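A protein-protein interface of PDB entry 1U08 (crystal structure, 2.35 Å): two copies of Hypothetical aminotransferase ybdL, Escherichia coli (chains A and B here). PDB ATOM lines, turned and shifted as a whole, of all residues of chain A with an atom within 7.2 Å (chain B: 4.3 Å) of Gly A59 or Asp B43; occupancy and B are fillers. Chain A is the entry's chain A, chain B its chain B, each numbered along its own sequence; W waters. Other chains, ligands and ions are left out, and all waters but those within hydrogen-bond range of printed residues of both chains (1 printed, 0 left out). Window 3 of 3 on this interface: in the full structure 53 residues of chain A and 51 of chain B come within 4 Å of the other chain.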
ATOM      1  N   ALA A  53      33.778  17.552 -24.063  1.00  0.00           N
ATOM      2  CA  ALA A  53      33.053  16.855 -22.997  1.00  0.00           C
ATOM      3  C   ALA A  53      33.517  17.308 -21.617  1.00  0.00           C
ATOM      4  O   ALA A  53      32.717  17.430 -20.690  1.00  0.00           O
ATOM      5  CB  ALA A  53      33.231  15.338 -23.140  1.00  0.00           C
ATOM      6  N   HIS A  54      34.810  17.559 -21.487  1.00  0.00           N
ATOM      7  CA  HIS A  54      35.367  17.998 -20.220  1.00  0.00           C
ATOM      8  C   HIS A  54      34.756  19.331 -19.784  1.00  0.00           C
ATOM      9  O   HIS A  54      34.280  19.468 -18.663  1.00  0.00           O
ATOM     10  CB  HIS A  54      36.891  18.120 -20.332  1.00  0.00           C
ATOM     11  CG  HIS A  54      37.535  18.771 -19.147  1.00  0.00           C
ATOM     12  ND1 HIS A  54      37.909  20.099 -19.138  1.00  0.00           N
ATOM     13  CD2 HIS A  54      37.869  18.278 -17.932  1.00  0.00           C
ATOM     14  CE1 HIS A  54      38.449  20.394 -17.969  1.00  0.00           C
ATOM     15  NE2 HIS A  54      38.435  19.306 -17.218  1.00  0.00           N
ATOM     16  N   HIS A  55      34.749  20.309 -20.677  1.00  0.00           N
ATOM     17  CA  HIS A  55      34.194  21.600 -20.331  1.00  0.00           C
ATOM     18  C   HIS A  55      32.693  21.580 -20.098  1.00  0.00           C
ATOM     19  O   HIS A  55      32.174  22.323 -19.260  1.00  0.00           O
ATOM     20  CB  HIS A  55      34.591  22.617 -21.391  1.00  0.00           C
ATOM     21  CG  HIS A  55      36.048  22.932 -21.357  1.00  0.00           C
ATOM     22  ND1 HIS A  55      36.634  23.568 -20.285  1.00  0.00           N
ATOM     23  CD2 HIS A  55      37.053  22.624 -22.210  1.00  0.00           C
ATOM     24  CE1 HIS A  55      37.939  23.637 -20.480  1.00  0.00           C
ATOM     25  NE2 HIS A  55      38.218  23.070 -21.640  1.00  0.00           N
ATOM     26  N   VAL A  56      31.996  20.726 -20.832  1.00  0.00           N
ATOM     27  CA  VAL A  56      30.561  20.593 -20.650  1.00  0.00           C
ATOM     28  C   VAL A  56      30.324  20.029 -19.244  1.00  0.00           C
ATOM     29  O   VAL A  56      29.434  20.472 -18.521  1.00  0.00           O
ATOM     30  CB  VAL A  56      29.973  19.635 -21.699  1.00  0.00           C
ATOM     31  CG1 VAL A  56      28.536  19.289 -21.356  1.00  0.00           C
ATOM     32  CG2 VAL A  56      30.037  20.282 -23.061  1.00  0.00           C
ATOM     33  N   ALA A  57      31.152  19.065 -18.859  1.00  0.00           N
ATOM     34  CA  ALA A  57      31.037  18.429 -17.555  1.00  0.00           C
ATOM     35  C   ALA A  57      31.399  19.373 -16.406  1.00  0.00           C
ATOM     36  O   ALA A  57      30.831  19.272 -15.319  1.00  0.00           O
ATOM     37  CB  ALA A  57      31.910  17.182 -17.513  1.00  0.00           C
ATOM     38  N   GLN A  58      32.338  20.287 -16.643  1.00  0.00           N
ATOM     39  CA  GLN A  58      32.735  21.236 -15.610  1.00  0.00           C
ATOM     40  C   GLN A  58      31.746  22.385 -15.458  1.00  0.00           C
ATOM     41  O   GLN A  58      31.980  23.301 -14.667  1.00  0.00           O
ATOM     42  CB  GLN A  58      34.125  21.813 -15.893  1.00  0.00           C
ATOM     43  CG  GLN A  58      35.270  20.893 -15.512  1.00  0.00           C
ATOM     44  CD  GLN A  58      36.560  21.651 -15.257  1.00  0.00           C
ATOM     45  OE1 GLN A  58      37.078  22.352 -16.137  1.00  0.00           O
ATOM     46  NE2 GLN A  58      37.088  21.515 -14.043  1.00  0.00           N
ATOM     47  N   GLY A  59      30.656  22.349 -16.223  1.00  0.00           N
ATOM     48  CA  GLY A  59      29.647  23.396 -16.129  1.00  0.00           C
ATOM     49  C   GLY A  59      29.901  24.694 -16.888  1.00  0.00           C
ATOM     50  O   GLY A  59      29.255  25.712 -16.614  1.00  0.00           O
ATOM     51  N   ALA A  60      30.836  24.679 -17.833  1.00  0.00           N
ATOM     52  CA  ALA A  60      31.120  25.873 -18.628  1.00  0.00           C
ATOM     53  C   ALA A  60      30.116  25.936 -19.789  1.00  0.00           C
ATOM     54  O   ALA A  60      30.502  25.909 -20.958  1.00  0.00           O
ATOM     55  CB  ALA A  60      32.540  25.813 -19.164  1.00  0.00           C
ATOM     56  N   ASN A  61      28.829  26.025 -19.459  1.00  0.00           N
ATOM     57  CA  ASN A  61      27.784  26.041 -20.477  1.00  0.00           C
ATOM     58  C   ASN A  61      26.908  27.291 -20.559  1.00  0.00           C
ATOM     59  O   ASN A  61      25.880  27.284 -21.240  1.00  0.00           O
ATOM     60  CB  ASN A  61      26.904  24.809 -20.295  1.00  0.00           C
ATOM     61  CG  ASN A  61      27.711  23.530 -20.257  1.00  0.00           C
ATOM     62  OD1 ASN A  61      28.436  23.211 -21.202  1.00  0.00           O
ATOM     63  ND2 ASN A  61      27.596  22.792 -19.163  1.00  0.00           N
ATOM     64  N   GLN A  62      27.304  28.357 -19.872  1.00  0.00           N
ATOM     65  CA  GLN A  62      26.544  29.603 -19.908  1.00  0.00           C
ATOM     66  C   GLN A  62      27.241  30.525 -20.907  1.00  0.00           C
ATOM     67  O   GLN A  62      28.357  30.241 -21.323  1.00  0.00           O
ATOM     68  CB  GLN A  62      26.496  30.254 -18.514  1.00  0.00           C
ATOM     69  CG  GLN A  62      25.884  29.367 -17.414  1.00  0.00           C
ATOM     70  CD  GLN A  62      24.566  28.706 -17.833  1.00  0.00           C
ATOM     71  OE1 GLN A  62      23.680  29.350 -18.400  1.00  0.00           O
ATOM     72  NE2 GLN A  62      24.435  27.419 -17.540  1.00  0.00           N
ATOM     73  N   THR A 271      30.143  27.998 -25.852  1.00  0.00           N
ATOM     74  CA  THR A 271      31.188  28.164 -24.847  1.00  0.00           C
ATOM     75  C   THR A 271      32.119  26.974 -24.621  1.00  0.00           C
ATOM     76  O   THR A 271      33.346  27.117 -24.626  1.00  0.00           O
ATOM     77  CB  THR A 271      30.575  28.562 -23.483  1.00  0.00           C
ATOM     78  OG1 THR A 271      29.733  29.699 -23.674  1.00  0.00           O
ATOM     79  CG2 THR A 271      31.668  28.914 -22.480  1.00  0.00           C
ATOM     80  N   PRO A 272      31.553  25.784 -24.391  1.00  0.00           N
ATOM     81  CA  PRO A 272      32.455  24.652 -24.173  1.00  0.00           C
ATOM     82  C   PRO A 272      33.308  24.318 -25.398  1.00  0.00           C
ATOM     83  O   PRO A 272      34.449  23.861 -25.260  1.00  0.00           O
ATOM     84  CB  PRO A 272      31.508  23.518 -23.752  1.00  0.00           C
ATOM     85  CG  PRO A 272      30.168  23.932 -24.338  1.00  0.00           C
ATOM     86  CD  PRO A 272      30.154  25.413 -24.112  1.00  0.00           C
ATOM     87  N   PHE B  42      23.762  27.800 -12.166  1.00  0.00           N
ATOM     88  CA  PHE B  42      23.691  26.369 -11.915  1.00  0.00           C
ATOM     89  C   PHE B  42      23.697  25.750 -13.316  1.00  0.00           C
ATOM     90  O   PHE B  42      23.468  26.442 -14.304  1.00  0.00           O
ATOM     91  CB  PHE B  42      22.434  25.982 -11.109  1.00  0.00           C
ATOM     92  CG  PHE B  42      21.144  26.511 -11.667  1.00  0.00           C
ATOM     93  CD1 PHE B  42      20.543  25.910 -12.769  1.00  0.00           C
ATOM     94  CD2 PHE B  42      20.529  27.615 -11.090  1.00  0.00           C
ATOM     95  CE1 PHE B  42      19.346  26.403 -13.288  1.00  0.00           C
ATOM     96  CE2 PHE B  42      19.334  28.118 -11.600  1.00  0.00           C
ATOM     97  CZ  PHE B  42      18.743  27.511 -12.701  1.00  0.00           C
ATOM     98  N   ASP B  43      23.968  24.459 -13.417  1.00  0.00           N
ATOM     99  CA  ASP B  43      24.045  23.834 -14.729  1.00  0.00           C
ATOM    100  C   ASP B  43      22.775  23.124 -15.206  1.00  0.00           C
ATOM    101  O   ASP B  43      21.819  22.954 -14.449  1.00  0.00           O
ATOM    102  CB  ASP B  43      25.228  22.866 -14.741  1.00  0.00           C
ATOM    103  CG  ASP B  43      25.893  22.779 -16.094  1.00  0.00           C
ATOM    104  OD1 ASP B  43      26.249  23.834 -16.652  1.00  0.00           O
ATOM    105  OD2 ASP B  43      26.067  21.653 -16.589  1.00  0.00           O
ATOM    106  N   GLY B  44      22.791  22.709 -16.472  1.00  0.00           N
ATOM    107  CA  GLY B  44      21.656  22.026 -17.069  1.00  0.00           C
ATOM    108  C   GLY B  44      21.616  20.523 -16.853  1.00  0.00           C
ATOM    109  O   GLY B  44      22.461  19.969 -16.146  1.00  0.00           O
ATOM    110  N   GLN B  49      23.824  16.753 -21.736  1.00  0.00           N
ATOM    111  CA  GLN B  49      25.280  16.823 -21.871  1.00  0.00           C
ATOM    112  C   GLN B  49      25.809  15.479 -22.347  1.00  0.00           C
ATOM    113  O   GLN B  49      26.717  15.413 -23.172  1.00  0.00           O
ATOM    114  CB  GLN B  49      25.954  17.164 -20.540  1.00  0.00           C
ATOM    115  CG  GLN B  49      25.302  18.280 -19.766  1.00  0.00           C
ATOM    116  CD  GLN B  49      26.170  18.765 -18.618  1.00  0.00           C
ATOM    117  OE1 GLN B  49      26.857  17.986 -17.963  1.00  0.00           O
ATOM    118  NE2 GLN B  49      26.134  20.058 -18.367  1.00  0.00           N
ATOM    119  N   HIS B 239      18.720  25.573 -19.258  1.00  0.00           N
ATOM    120  CA  HIS B 239      19.720  26.159 -18.381  1.00  0.00           C
ATOM    121  C   HIS B 239      21.145  26.148 -18.923  1.00  0.00           C
ATOM    122  O   HIS B 239      22.097  26.092 -18.150  1.00  0.00           O
ATOM    123  CB  HIS B 239      19.704  25.433 -17.034  1.00  0.00           C
ATOM    124  CG  HIS B 239      18.337  25.038 -16.575  1.00  0.00           C
ATOM    125  ND1 HIS B 239      17.297  25.939 -16.468  1.00  0.00           N
ATOM    126  CD2 HIS B 239      17.843  23.842 -16.178  1.00  0.00           C
ATOM    127  CE1 HIS B 239      16.220  25.312 -16.023  1.00  0.00           C
ATOM    128  NE2 HIS B 239      16.524  24.040 -15.840  1.00  0.00           N
HETATM  129  O   HOH W   1      26.599  26.357 -15.980  1.00  0.00           O
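The side-chain amide nitrogen of Asn A61 sits close to the side-chain amide nitrogen of Gln B49 (3.2 Å).
OD1 of Asp B43 is in hydrogen-bond range of ND2 of Asn A61 (3.0 Å).
O of His B239 is in hydrogen-bond range of NE2 of Gln A62, 2.8 Å away.
The backbone carbonyl oxygen of Val A56 is in hydrogen-bond range of the side-chain amide nitrogen of Gln B49, 3.3 Å away.
The side-chain amide nitrogen (ND2) of Asn A61 sits at hydrogen-bond distance from the backbone carbonyl oxygen (O) of Val A56.
The backbone carbonyl oxygen of Gln A62 sits at hydrogen-bond distance from the side-chain hydroxyl of Thr A271 (2.8 Å).
OD1 of Asp B43 touches CA of Gly A59 (3.5 Å).
NE2 of Gln A62 touches O of Phe B42 (3.5 Å).
Ala A53 touches none of the printed residues of chain B.
Gly A59 touches one residue of chain B.
Of the printed residues of chain B, Asn A61 touches Asp B43 and Gln B49.
Pro A272 touches none of the printed residues of chain B.
Of the printed residues of chain A, Phe B42 touches Gln A62 (3.5 Å).
Asp B43 touches two residues of chain A.
Printed residues of chain A within 4 Å of His B239: Gln A62.
The nearest residue of chain A that does not touch Asp B43 is Val A56 (4.1 Å).
Hydrophobic or aromatic side chains of chain A that line the printed part of chain B: Val A56.
Among the printed residues, 6 pairs touch across the chains.
Among the printed residues, no Asp or Glu carboxylate lies within 4 Å of a Lys or Arg side-chain nitrogen of the other chain.
No position is printed for both chains.
Of the 6 pairs that touch across the chains among the printed residues, none has its exchanged pair printed and touching as well.
Water W1 lies within hydrogen-bond range of OD1 of Asp B43 (2.6 Å), O of Gly A59 (2.8 Å) and NE2 of Gln A62 (2.9 Å).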
